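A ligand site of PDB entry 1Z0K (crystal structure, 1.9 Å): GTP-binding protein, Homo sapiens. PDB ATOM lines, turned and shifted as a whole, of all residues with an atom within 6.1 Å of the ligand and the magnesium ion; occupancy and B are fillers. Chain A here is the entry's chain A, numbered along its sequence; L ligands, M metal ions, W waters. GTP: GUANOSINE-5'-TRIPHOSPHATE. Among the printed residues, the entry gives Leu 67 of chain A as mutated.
The side-chain hydroxyl (OG) of Ser 37 sits at hydrogen-bond distance from an oxygen (O2A) of the ligand (2.9 Å). NZ of Lys 122 is in hydrogen-bond range of O4' of the ligand (3.2 Å). A nitrogen (N7) of the ligand sits at hydrogen-bond distance from the side-chain amide nitrogen (ND2) of Asn 121 (3.2 Å). O1A of the ligand lies within hydrogen-bond range of N of Ser 22, 3.2 Å away. The side-chain hydroxyl of Thr 19 sits at hydrogen-bond distance from an oxygen (O1B) of the ligand (3.5 Å). The backbone NH (N) of Gly 66 lies within hydrogen-bond range of an oxygen (O3G) of the ligand (2.7 Å). N of Cys 23 sits at hydrogen-bond distance from O1A of the ligand, 2.9 Å away. OD1 of Asp 124 is in hydrogen-bond range of N1 of the ligand, 2.7 Å away. N of Ala 152 is in hydrogen-bond range of O6 of the ligand, at 2.8 Å. O1A of the ligand lies within hydrogen-bond range of SG of Cys 23. The side-chain amino group (NZ) of Lys 21 is in salt-bridge range of an oxygen (O1B) of the ligand, at 2.7 Å. An oxygen (O2G) of the ligand lies close to the backbone NH of Thr 40, at 2.5 Å. N of Thr 19 sits at hydrogen-bond distance from O1B of the ligand, 3.4 Å away. An oxygen (O1B) of the ligand lies within hydrogen-bond range of the backbone NH (N) of Lys 21 (2.8 Å). N of Gly 18 is in hydrogen-bond range of O3B of the ligand (2.9 Å). O1B of the ligand lies within hydrogen-bond range of N of Gly 20 (3.0 Å). An oxygen (O6) of the ligand lies within hydrogen-bond range of the backbone NH (N) of Leu 153, at 3.3 Å.
The side-chain amino group of Lys 122 sits at hydrogen-bond distance from the backbone carbonyl oxygen of Gly 18 (2.8 Å). N of Leu 153 sits close to OG of Ser 151 (3.3 Å). The side-chain hydroxyl (OG) of Ser 37 sits at hydrogen-bond distance from the side-chain sulfur (SG) of Cys 23. The side-chain amide nitrogen (ND2) of Asn 121 is in hydrogen-bond range of the backbone carbonyl oxygen (O) of Thr 19 (3.0 Å). The side-chain hydroxyl (OG) of Ser 22 lies close to the side-chain carboxylate (OD2) of Asp 63. The backbone NH (N) of Lys 122 sits at hydrogen-bond distance from the backbone carbonyl oxygen (O) of Thr 150, at 3.1 Å. The side-chain carboxylate (OE1) of Glu 44 sits close to the side-chain hydroxyl (OG) of Ser 22. The side-chain carboxylate (OE1) of Glu 44 sits close to the side-chain hydroxyl (OG1) of Thr 40 (3.5 Å).
Merely in contact with the ligand: Asn 16 (3.8 Å), Ala 17 (3.3 Å), Phe 33 (3.2 Å), His 39 (3.5 Å), Thr 64 (3.8 Å), Ala 65 (3.6 Å), Leu 67 (3.9 Å), Leu 125 (3.4 Å) and Ser 151 (3.5 Å). Hydrophobic or aromatic side chains that line the ligand: Ala 17, Phe 33, His 39, Leu 67, Leu 125, Ala 152 and Leu 153. Within 4 Å of the ligand: Asn 16, Ala 17, Gly 18, Thr 19, Gly 20, Lys 21, Ser 22, Cys 23, Phe 33, Ser 37, His 39, Thr 40, Thr 64, Ala 65, Gly 66, Leu 67, Asn 121, Lys 122, Asp 124, Leu 125, Ser 151, Ala 152 and Leu 153.
Asp 63 touches the magnesium ion (OD2 to MG, 3.9 Å). Three residues have an atom within 4 Å of the magnesium ion: Ser 22, Thr 40 and Asp 63. The nearest printed residue that does not touch the magnesium ion is Thr 64 (4.4 Å).
The magnesium ion is bound by O2B of the ligand (1.8 Å), water W2 (1.9 Å), O2G of the ligand (2.1 Å), OG of Ser 22 (2.2 Å), OG1 of Thr 40 (2.3 Å) and water W4 (2.4 Å).
Water W2 lies within hydrogen-bond range of OD1 of Asp 63 (2.6 Å), O of Thr 64 (2.6 Å) and O3G of the ligand (3.5 Å). Water W4 lies within hydrogen-bond range of O2A of the ligand (2.7 Å), O of Asn 38 (2.7 Å) and N of Thr 40 (3.2 Å). Water W1 lies within hydrogen-bond range of O1G of the ligand (2.7 Å), O of Thr 40 (3.0 Å), N of Leu 67 (3.1 Å) and N of Gly 66 (3.3 Å). Water W6 bridges O2A of the ligand and N of His 39. Water W7 lies within hydrogen-bond range of the side-chain amino group (NZ) of Lys 122 (2.6 Å) and an oxygen (O4') of the ligand (3.4 Å).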
ATOM      1  N   GLY A  15     -16.256   4.093  16.334  1.00  0.00           N
ATOM      2  CA  GLY A  15     -17.494   3.337  16.531  1.00  0.00           C
ATOM      3  C   GLY A  15     -18.717   4.214  16.366  1.00  0.00           C
ATOM      4  O   GLY A  15     -18.604   5.437  16.263  1.00  0.00           O
ATOM      5  N   ASN A  16     -19.891   3.588  16.307  1.00  0.00           N
ATOM      6  CA  ASN A  16     -21.134   4.333  16.104  1.00  0.00           C
ATOM      7  C   ASN A  16     -21.357   5.467  17.089  1.00  0.00           C
ATOM      8  O   ASN A  16     -20.920   5.414  18.237  1.00  0.00           O
ATOM      9  CB  ASN A  16     -22.331   3.368  16.120  1.00  0.00           C
ATOM     10  CG  ASN A  16     -22.715   2.906  14.734  1.00  0.00           C
ATOM     11  OD1 ASN A  16     -21.859   2.711  13.862  1.00  0.00           O
ATOM     12  ND2 ASN A  16     -24.021   2.729  14.508  1.00  0.00           N
ATOM     13  N   ALA A  17     -22.048   6.514  16.641  1.00  0.00           N
ATOM     14  CA  ALA A  17     -22.476   7.594  17.512  1.00  0.00           C
ATOM     15  C   ALA A  17     -23.232   7.025  18.695  1.00  0.00           C
ATOM     16  O   ALA A  17     -23.968   6.050  18.547  1.00  0.00           O
ATOM     17  CB  ALA A  17     -23.340   8.568  16.755  1.00  0.00           C
ATOM     18  N   GLY A  18     -23.022   7.600  19.876  1.00  0.00           N
ATOM     19  CA  GLY A  18     -23.750   7.196  21.069  1.00  0.00           C
ATOM     20  C   GLY A  18     -23.223   5.969  21.790  1.00  0.00           C
ATOM     21  O   GLY A  18     -23.719   5.627  22.857  1.00  0.00           O
ATOM     22  N   THR A  19     -22.203   5.311  21.229  1.00  0.00           N
ATOM     23  CA  THR A  19     -21.630   4.114  21.850  1.00  0.00           C
ATOM     24  C   THR A  19     -20.878   4.395  23.165  1.00  0.00           C
ATOM     25  O   THR A  19     -20.663   3.483  23.973  1.00  0.00           O
ATOM     26  CB  THR A  19     -20.722   3.322  20.893  1.00  0.00           C
ATOM     27  OG1 THR A  19     -19.725   4.188  20.325  1.00  0.00           O
ATOM     28  CG2 THR A  19     -21.553   2.702  19.771  1.00  0.00           C
ATOM     29  N   GLY A  20     -20.487   5.647  23.373  1.00  0.00           N
ATOM     30  CA  GLY A  20     -19.839   6.060  24.605  1.00  0.00           C
ATOM     31  C   GLY A  20     -18.343   6.343  24.471  1.00  0.00           C
ATOM     32  O   GLY A  20     -17.605   6.255  25.451  1.00  0.00           O
ATOM     33  N   LYS A  21     -17.916   6.707  23.267  1.00  0.00           N
ATOM     34  CA  LYS A  21     -16.496   6.942  22.988  1.00  0.00           C
ATOM     35  C   LYS A  21     -15.909   8.080  23.802  1.00  0.00           C
ATOM     36  O   LYS A  21     -14.837   7.938  24.405  1.00  0.00           O
ATOM     37  CB  LYS A  21     -16.287   7.138  21.474  1.00  0.00           C
ATOM     38  CG  LYS A  21     -16.750   5.941  20.643  1.00  0.00           C
ATOM     39  CD  LYS A  21     -16.442   6.073  19.166  1.00  0.00           C
ATOM     40  CE  LYS A  21     -17.182   7.215  18.482  1.00  0.00           C
ATOM     41  NZ  LYS A  21     -18.657   7.139  18.724  1.00  0.00           N
ATOM     42  N   SER A  22     -16.623   9.215  23.861  1.00  0.00           N
ATOM     43  CA  SER A  22     -16.141  10.377  24.595  1.00  0.00           C
ATOM     44  C   SER A  22     -16.149  10.109  26.087  1.00  0.00           C
ATOM     45  O   SER A  22     -15.229  10.503  26.785  1.00  0.00           O
ATOM     46  CB  SER A  22     -16.981  11.615  24.278  1.00  0.00           C
ATOM     47  OG  SER A  22     -16.972  11.826  22.867  1.00  0.00           O
ATOM     48  N   CYS A  23     -17.184   9.424  26.564  1.00  0.00           N
ATOM     49  CA  CYS A  23     -17.242   9.040  27.969  1.00  0.00           C
ATOM     50  C   CYS A  23     -16.107   8.088  28.385  1.00  0.00           C
ATOM     51  O   CYS A  23     -15.582   8.197  29.482  1.00  0.00           O
ATOM     52  CB  CYS A  23     -18.613   8.451  28.309  1.00  0.00           C
ATOM     53  SG  CYS A  23     -19.875   9.728  28.366  1.00  0.00           S
ATOM     54  N   LEU A  24     -15.732   7.169  27.500  1.00  0.00           N
ATOM     55  CA  LEU A  24     -14.577   6.293  27.730  1.00  0.00           C
ATOM     56  C   LEU A  24     -13.284   7.096  27.861  1.00  0.00           C
ATOM     57  O   LEU A  24     -12.479   6.866  28.778  1.00  0.00           O
ATOM     58  CB  LEU A  24     -14.461   5.272  26.598  1.00  0.00           C
ATOM     59  CG  LEU A  24     -15.433   4.084  26.607  1.00  0.00           C
ATOM     60  CD1 LEU A  24     -15.238   3.267  25.343  1.00  0.00           C
ATOM     61  CD2 LEU A  24     -15.269   3.209  27.859  1.00  0.00           C
ATOM     62  N   PHE A  33     -17.259   9.838  35.334  1.00  0.00           N
ATOM     63  CA  PHE A  33     -18.265   9.709  34.288  1.00  0.00           C
ATOM     64  C   PHE A  33     -18.777  11.087  33.907  1.00  0.00           C
ATOM     65  O   PHE A  33     -19.333  11.816  34.736  1.00  0.00           O
ATOM     66  CB  PHE A  33     -19.407   8.789  34.718  1.00  0.00           C
ATOM     67  CG  PHE A  33     -20.399   8.508  33.621  1.00  0.00           C
ATOM     68  CD1 PHE A  33     -19.968   8.062  32.362  1.00  0.00           C
ATOM     69  CD2 PHE A  33     -21.768   8.689  33.829  1.00  0.00           C
ATOM     70  CE1 PHE A  33     -20.873   7.794  31.354  1.00  0.00           C
ATOM     71  CE2 PHE A  33     -22.690   8.425  32.819  1.00  0.00           C
ATOM     72  CZ  PHE A  33     -22.236   7.969  31.586  1.00  0.00           C
ATOM     73  N   LYS A  34     -18.550  11.415  32.640  1.00  0.00           N
ATOM     74  CA  LYS A  34     -18.915  12.677  32.017  1.00  0.00           C
ATOM     75  C   LYS A  34     -20.418  12.947  32.152  1.00  0.00           C
ATOM     76  O   LYS A  34     -21.243  12.199  31.634  1.00  0.00           O
ATOM     77  CB  LYS A  34     -18.493  12.584  30.539  1.00  0.00           C
ATOM     78  CG  LYS A  34     -18.576  13.845  29.723  1.00  0.00           C
ATOM     79  CD  LYS A  34     -18.009  13.582  28.329  1.00  0.00           C
ATOM     80  CE  LYS A  34     -18.310  14.725  27.368  1.00  0.00           C
ATOM     81  NZ  LYS A  34     -17.906  16.054  27.931  1.00  0.00           N
ATOM     82  N   ASP A  35     -20.766  14.022  32.867  1.00  0.00           N
ATOM     83  CA  ASP A  35     -22.168  14.380  33.130  1.00  0.00           C
ATOM     84  C   ASP A  35     -22.880  15.056  31.948  1.00  0.00           C
ATOM     85  O   ASP A  35     -24.004  14.690  31.584  1.00  0.00           O
ATOM     86  CB  ASP A  35     -22.299  15.216  34.422  1.00  0.00           C
ATOM     87  CG  ASP A  35     -21.454  16.503  34.406  1.00  0.00           C
ATOM     88  OD1 ASP A  35     -20.682  16.754  33.449  1.00  0.00           O
ATOM     89  OD2 ASP A  35     -21.578  17.274  35.375  1.00  0.00           O
ATOM     90  N   SER A  37     -22.878  15.170  28.355  1.00  0.00           N
ATOM     91  CA  SER A  37     -22.437  14.555  27.102  1.00  0.00           C
ATOM     92  C   SER A  37     -23.393  14.840  25.964  1.00  0.00           C
ATOM     93  O   SER A  37     -24.623  14.859  26.147  1.00  0.00           O
ATOM     94  CB  SER A  37     -22.175  13.048  27.253  1.00  0.00           C
ATOM     95  OG  SER A  37     -21.116  12.647  26.406  1.00  0.00           O
ATOM     96  N   ASN A  38     -22.812  15.086  24.794  1.00  0.00           N
ATOM     97  CA  ASN A  38     -23.551  15.356  23.580  1.00  0.00           C
ATOM     98  C   ASN A  38     -22.716  14.838  22.421  1.00  0.00           C
ATOM     99  O   ASN A  38     -21.484  14.763  22.514  1.00  0.00           O
ATOM    100  CB  ASN A  38     -23.825  16.837  23.434  1.00  0.00           C
ATOM    101  N   HIS A  39     -23.390  14.494  21.326  1.00  0.00           N
ATOM    102  CA  HIS A  39     -22.752  13.987  20.112  1.00  0.00           C
ATOM    103  C   HIS A  39     -21.449  14.736  19.805  1.00  0.00           C
ATOM    104  O   HIS A  39     -21.449  15.973  19.765  1.00  0.00           O
ATOM    105  CB  HIS A  39     -23.701  14.086  18.950  1.00  0.00           C
ATOM    106  N   THR A  40     -20.363  13.992  19.614  1.00  0.00           N
ATOM    107  CA  THR A  40     -19.068  14.609  19.322  1.00  0.00           C
ATOM    108  C   THR A  40     -19.120  15.385  18.038  1.00  0.00           C
ATOM    109  O   THR A  40     -19.593  14.913  17.003  1.00  0.00           O
ATOM    110  CB  THR A  40     -17.865  13.622  19.356  1.00  0.00           C
ATOM    111  OG1 THR A  40     -17.506  13.397  20.722  1.00  0.00           O
ATOM    112  CG2 THR A  40     -16.636  14.185  18.611  1.00  0.00           C
ATOM    113  N   ILE A  41     -18.639  16.612  18.164  1.00  0.00           N
ATOM    114  CA  ILE A  41     -18.830  17.636  17.192  1.00  0.00           C
ATOM    115  C   ILE A  41     -17.575  17.695  16.319  1.00  0.00           C
ATOM    116  O   ILE A  41     -17.099  18.752  15.899  1.00  0.00           O
ATOM    117  CB  ILE A  41     -19.280  18.945  17.946  1.00  0.00           C
ATOM    118  CG1 ILE A  41     -20.780  18.846  18.285  1.00  0.00           C
ATOM    119  CG2 ILE A  41     -18.995  20.210  17.163  1.00  0.00           C
ATOM    120  CD1 ILE A  41     -21.643  18.267  17.155  1.00  0.00           C
ATOM    121  N   GLU A  44     -12.474  14.736  19.354  1.00  0.00           N
ATOM    122  CA  GLU A  44     -11.860  15.203  20.600  1.00  0.00           C
ATOM    123  C   GLU A  44     -10.433  14.692  20.743  1.00  0.00           C
ATOM    124  O   GLU A  44     -10.076  13.657  20.167  1.00  0.00           O
ATOM    125  CB  GLU A  44     -12.651  14.732  21.817  1.00  0.00           C
ATOM    126  CG  GLU A  44     -13.851  15.576  22.163  1.00  0.00           C
ATOM    127  CD  GLU A  44     -14.516  15.123  23.457  1.00  0.00           C
ATOM    128  OE1 GLU A  44     -15.666  14.634  23.371  1.00  0.00           O
ATOM    129  OE2 GLU A  44     -13.900  15.246  24.544  1.00  0.00           O
ATOM    130  N   ASP A  63     -10.504  10.880  19.795  1.00  0.00           N
ATOM    131  CA  ASP A  63     -11.864  10.367  19.991  1.00  0.00           C
ATOM    132  C   ASP A  63     -12.760  10.897  18.875  1.00  0.00           C
ATOM    133  O   ASP A  63     -13.173  12.065  18.887  1.00  0.00           O
ATOM    134  CB  ASP A  63     -12.389  10.797  21.361  1.00  0.00           C
ATOM    135  CG  ASP A  63     -13.897  10.650  21.489  1.00  0.00           C
ATOM    136  OD1 ASP A  63     -14.448   9.630  21.027  1.00  0.00           O
ATOM    137  OD2 ASP A  63     -14.516  11.565  22.071  1.00  0.00           O
ATOM    138  N   THR A  64     -13.058  10.027  17.913  1.00  0.00           N
ATOM    139  CA  THR A  64     -13.715  10.425  16.676  1.00  0.00           C
ATOM    140  C   THR A  64     -15.231  10.518  16.834  1.00  0.00           C
ATOM    141  O   THR A  64     -15.790   9.963  17.784  1.00  0.00           O
ATOM    142  CB  THR A  64     -13.357   9.480  15.506  1.00  0.00           C
ATOM    143  OG1 THR A  64     -13.913   8.173  15.735  1.00  0.00           O
ATOM    144  CG2 THR A  64     -11.840   9.362  15.320  1.00  0.00           C
ATOM    145  N   ALA A  65     -15.891  11.210  15.909  1.00  0.00           N
ATOM    146  CA  ALA A  65     -17.357  11.296  15.905  1.00  0.00           C
ATOM    147  C   ALA A  65     -17.929  10.125  15.130  1.00  0.00           C
ATOM    148  O   ALA A  65     -17.427   9.794  14.057  1.00  0.00           O
ATOM    149  CB  ALA A  65     -17.796  12.590  15.266  1.00  0.00           C
ATOM    150  N   GLY A  66     -18.964   9.501  15.671  1.00  0.00           N
ATOM    151  CA  GLY A  66     -19.669   8.415  14.982  1.00  0.00           C
ATOM    152  C   GLY A  66     -20.763   8.879  14.021  1.00  0.00           C
ATOM    153  O   GLY A  66     -21.177   8.111  13.142  1.00  0.00           O
ATOM    154  N   LEU A  67     -21.214  10.123  14.176  1.00  0.00           N
ATOM    155  CA  LEU A  67     -22.297  10.657  13.317  1.00  0.00           C
ATOM    156  C   LEU A  67     -21.904  10.717  11.852  1.00  0.00           C
ATOM    157  O   LEU A  67     -20.768  11.056  11.512  1.00  0.00           O
ATOM    158  CB  LEU A  67     -22.694  12.054  13.776  1.00  0.00           C
ATOM    159  CG  LEU A  67     -23.214  12.177  15.204  1.00  0.00           C
ATOM    160  CD1 LEU A  67     -23.577  13.628  15.525  1.00  0.00           C
ATOM    161  CD2 LEU A  67     -24.416  11.274  15.419  1.00  0.00           C
ATOM    162  N   ASN A 121     -19.092  -1.519  25.235  1.00  0.00           N
ATOM    163  CA  ASN A 121     -19.306  -0.529  26.254  1.00  0.00           C
ATOM    164  C   ASN A 121     -20.720  -0.522  26.833  1.00  0.00           C
ATOM    165  O   ASN A 121     -21.635  -1.120  26.242  1.00  0.00           O
ATOM    166  CB  ASN A 121     -18.935   0.865  25.739  1.00  0.00           C
ATOM    167  CG  ASN A 121     -18.861   1.875  26.847  1.00  0.00           C
ATOM    168  OD1 ASN A 121     -18.293   1.605  27.896  1.00  0.00           O
ATOM    169  ND2 ASN A 121     -19.453   3.033  26.641  1.00  0.00           N
ATOM    170  N   LYS A 122     -20.870   0.167  27.958  1.00  0.00           N
ATOM    171  CA  LYS A 122     -22.119   0.276  28.742  1.00  0.00           C
ATOM    172  C   LYS A 122     -22.519  -1.065  29.365  1.00  0.00           C
ATOM    173  O   LYS A 122     -23.711  -1.386  29.477  1.00  0.00           O
ATOM    174  CB  LYS A 122     -23.282   0.868  27.923  1.00  0.00           C
ATOM    175  CG  LYS A 122     -22.930   2.139  27.147  1.00  0.00           C
ATOM    176  CD  LYS A 122     -24.203   2.790  26.593  1.00  0.00           C
ATOM    177  CE  LYS A 122     -23.872   3.900  25.606  1.00  0.00           C
ATOM    178  NZ  LYS A 122     -25.117   4.495  25.030  1.00  0.00           N
ATOM    179  N   LYS A 123     -21.521  -1.846  29.778  1.00  0.00           N
ATOM    180  CA  LYS A 123     -21.806  -3.164  30.360  1.00  0.00           C
ATOM    181  C   LYS A 123     -22.517  -3.054  31.712  1.00  0.00           C
ATOM    182  O   LYS A 123     -23.040  -4.044  32.223  1.00  0.00           O
ATOM    183  CB  LYS A 123     -20.546  -4.047  30.432  1.00  0.00           C
ATOM    184  CG  LYS A 123     -19.734  -3.920  31.704  1.00  0.00           C
ATOM    185  CD  LYS A 123     -18.628  -4.999  31.756  1.00  0.00           C
ATOM    186  CE  LYS A 123     -19.134  -6.309  32.370  1.00  0.00           C
ATOM    187  NZ  LYS A 123     -18.012  -7.219  32.718  1.00  0.00           N
ATOM    188  N   ASP A 124     -22.556  -1.844  32.278  1.00  0.00           N
ATOM    189  CA  ASP A 124     -23.284  -1.589  33.515  1.00  0.00           C
ATOM    190  C   ASP A 124     -24.802  -1.658  33.293  1.00  0.00           C
ATOM    191  O   ASP A 124     -25.572  -1.735  34.247  1.00  0.00           O
ATOM    192  CB  ASP A 124     -22.877  -0.237  34.093  1.00  0.00           C
ATOM    193  CG  ASP A 124     -23.161   0.915  33.143  1.00  0.00           C
ATOM    194  OD1 ASP A 124     -22.398   1.073  32.164  1.00  0.00           O
ATOM    195  OD2 ASP A 124     -24.133   1.667  33.372  1.00  0.00           O
ATOM    196  N   LEU A 125     -25.222  -1.610  32.027  1.00  0.00           N
ATOM    197  CA  LEU A 125     -26.634  -1.673  31.654  1.00  0.00           C
ATOM    198  C   LEU A 125     -26.981  -3.078  31.169  1.00  0.00           C
ATOM    199  O   LEU A 125     -27.549  -3.257  30.086  1.00  0.00           O
ATOM    200  CB  LEU A 125     -26.970  -0.633  30.579  1.00  0.00           C
ATOM    201  CG  LEU A 125     -26.653   0.843  30.825  1.00  0.00           C
ATOM    202  CD1 LEU A 125     -26.949   1.674  29.582  1.00  0.00           C
ATOM    203  CD2 LEU A 125     -27.390   1.409  32.053  1.00  0.00           C
ATOM    204  N   THR A 150     -16.723  -2.978  28.593  1.00  0.00           N
ATOM    205  CA  THR A 150     -16.309  -1.837  29.400  1.00  0.00           C
ATOM    206  C   THR A 150     -17.510  -1.069  29.957  1.00  0.00           C
ATOM    207  O   THR A 150     -18.628  -1.238  29.481  1.00  0.00           O
ATOM    208  CB  THR A 150     -15.449  -0.852  28.555  1.00  0.00           C
ATOM    209  OG1 THR A 150     -16.227  -0.368  27.458  1.00  0.00           O
ATOM    210  CG2 THR A 150     -14.234  -1.560  27.993  1.00  0.00           C
ATOM    211  N   SER A 151     -17.264  -0.248  30.967  1.00  0.00           N
ATOM    212  CA  SER A 151     -18.239   0.751  31.379  1.00  0.00           C
ATOM    213  C   SER A 151     -17.587   2.109  31.660  1.00  0.00           C
ATOM    214  O   SER A 151     -16.838   2.252  32.623  1.00  0.00           O
ATOM    215  CB  SER A 151     -19.015   0.289  32.620  1.00  0.00           C
ATOM    216  OG  SER A 151     -19.911   1.321  33.033  1.00  0.00           O
ATOM    217  N   ALA A 152     -17.882   3.105  30.834  1.00  0.00           N
ATOM    218  CA  ALA A 152     -17.390   4.468  31.075  1.00  0.00           C
ATOM    219  C   ALA A 152     -18.037   5.043  32.344  1.00  0.00           C
ATOM    220  O   ALA A 152     -17.463   5.929  32.987  1.00  0.00           O
ATOM    221  CB  ALA A 152     -17.664   5.357  29.872  1.00  0.00           C
ATOM    222  N   LEU A 153     -19.203   4.510  32.711  1.00  0.00           N
ATOM    223  CA  LEU A 153     -19.937   4.972  33.877  1.00  0.00           C
ATOM    224  C   LEU A 153     -19.307   4.527  35.196  1.00  0.00           C
ATOM    225  O   LEU A 153     -19.083   5.327  36.093  1.00  0.00           O
ATOM    226  CB  LEU A 153     -21.411   4.535  33.809  1.00  0.00           C
ATOM    227  CG  LEU A 153     -22.333   5.106  34.891  1.00  0.00           C
ATOM    228  CD1 LEU A 153     -23.754   5.232  34.382  1.00  0.00           C
ATOM    229  CD2 LEU A 153     -22.281   4.263  36.162  1.00  0.00           C
ATOM    230  N   THR A 154     -19.020   3.232  35.304  1.00  0.00           N
ATOM    231  CA  THR A 154     -18.380   2.692  36.504  1.00  0.00           C
ATOM    232  C   THR A 154     -16.854   2.687  36.418  1.00  0.00           C
ATOM    233  O   THR A 154     -16.180   2.566  37.436  1.00  0.00           O
ATOM    234  CB  THR A 154     -18.815   1.234  36.775  1.00  0.00           C
ATOM    235  OG1 THR A 154     -18.328   0.387  35.724  1.00  0.00           O
ATOM    236  CG2 THR A 154     -20.340   1.121  36.878  1.00  0.00           C
HETATM  237  PG  GTP L   1     -20.486  10.411  19.286  1.00  0.00           P
HETATM  238  O1G GTP L   1     -21.727  10.847  18.534  1.00  0.00           O
HETATM  239  O2G GTP L   1     -19.759  11.618  19.796  1.00  0.00           O
HETATM  240  O3G GTP L   1     -19.580   9.652  18.342  1.00  0.00           O
HETATM  241  O3B GTP L   1     -20.999   9.608  20.590  1.00  0.00           O
HETATM  242  PB  GTP L   1     -20.030   8.930  21.666  1.00  0.00           P
HETATM  243  O1B GTP L   1     -19.643   7.557  21.169  1.00  0.00           O
HETATM  244  O2B GTP L   1     -18.841   9.792  22.034  1.00  0.00           O
HETATM  245  O3A GTP L   1     -20.979   8.705  22.939  1.00  0.00           O
HETATM  246  PA  GTP L   1     -20.935   9.565  24.289  1.00  0.00           P
HETATM  247  O1A GTP L   1     -19.648   9.366  25.039  1.00  0.00           O
HETATM  248  O2A GTP L   1     -21.234  11.012  24.023  1.00  0.00           O
HETATM  249  O5' GTP L   1     -22.085   8.817  25.126  1.00  0.00           O
HETATM  250  C5' GTP L   1     -23.388   8.684  24.589  1.00  0.00           C
HETATM  251  C4' GTP L   1     -24.375   8.483  25.731  1.00  0.00           C
HETATM  252  O4' GTP L   1     -24.086   7.246  26.366  1.00  0.00           O
HETATM  253  C3' GTP L   1     -24.274   9.555  26.800  1.00  0.00           C
HETATM  254  O3' GTP L   1     -25.587   9.899  27.197  1.00  0.00           O
HETATM  255  C2' GTP L   1     -23.525   8.889  27.931  1.00  0.00           C
HETATM  256  O2' GTP L   1     -23.944   9.340  29.192  1.00  0.00           O
HETATM  257  C1' GTP L   1     -23.894   7.431  27.747  1.00  0.00           C
HETATM  258  N9  GTP L   1     -22.818   6.484  28.135  1.00  0.00           N
HETATM  259  C8  GTP L   1     -21.541   6.417  27.623  1.00  0.00           C
HETATM  260  N7  GTP L   1     -20.882   5.395  28.216  1.00  0.00           N
HETATM  261  C5  GTP L   1     -21.738   4.817  29.096  1.00  0.00           C
HETATM  262  C6  GTP L   1     -21.596   3.727  29.951  1.00  0.00           C
HETATM  263  O6  GTP L   1     -20.525   3.122  29.999  1.00  0.00           O
HETATM  264  N1  GTP L   1     -22.678   3.361  30.744  1.00  0.00           N
HETATM  265  C2  GTP L   1     -23.878   4.052  30.681  1.00  0.00           C
HETATM  266  N2  GTP L   1     -24.906   3.684  31.442  1.00  0.00           N
HETATM  267  N3  GTP L   1     -24.022   5.109  29.827  1.00  0.00           N
HETATM  268  C4  GTP L   1     -22.963   5.487  29.043  1.00  0.00           C
HETATM  269 MG    MG M   1     -18.260  11.280  21.164  1.00  0.00          MG
HETATM  270  O   HOH W   1     -20.695  12.226  16.430  1.00  0.00           O
HETATM  271  O   HOH W   2     -16.758  10.567  20.163  1.00  0.00           O
HETATM  272  O   HOH W   3     -26.015   9.713  30.450  1.00  0.00           O
HETATM  273  O   HOH W   4     -19.723  12.674  22.484  1.00  0.00           O
HETATM  274  O   HOH W   5     -27.322   4.914  31.685  1.00  0.00           O
HETATM  275  O   HOH W   6     -23.415  11.462  21.976  1.00  0.00           O
HETATM  276  O   HOH W   7     -26.733   5.134  27.005  1.00  0.00           O
HETATM  277  O   HOH W   8     -27.410   7.834  27.299  1.00  0.00           O
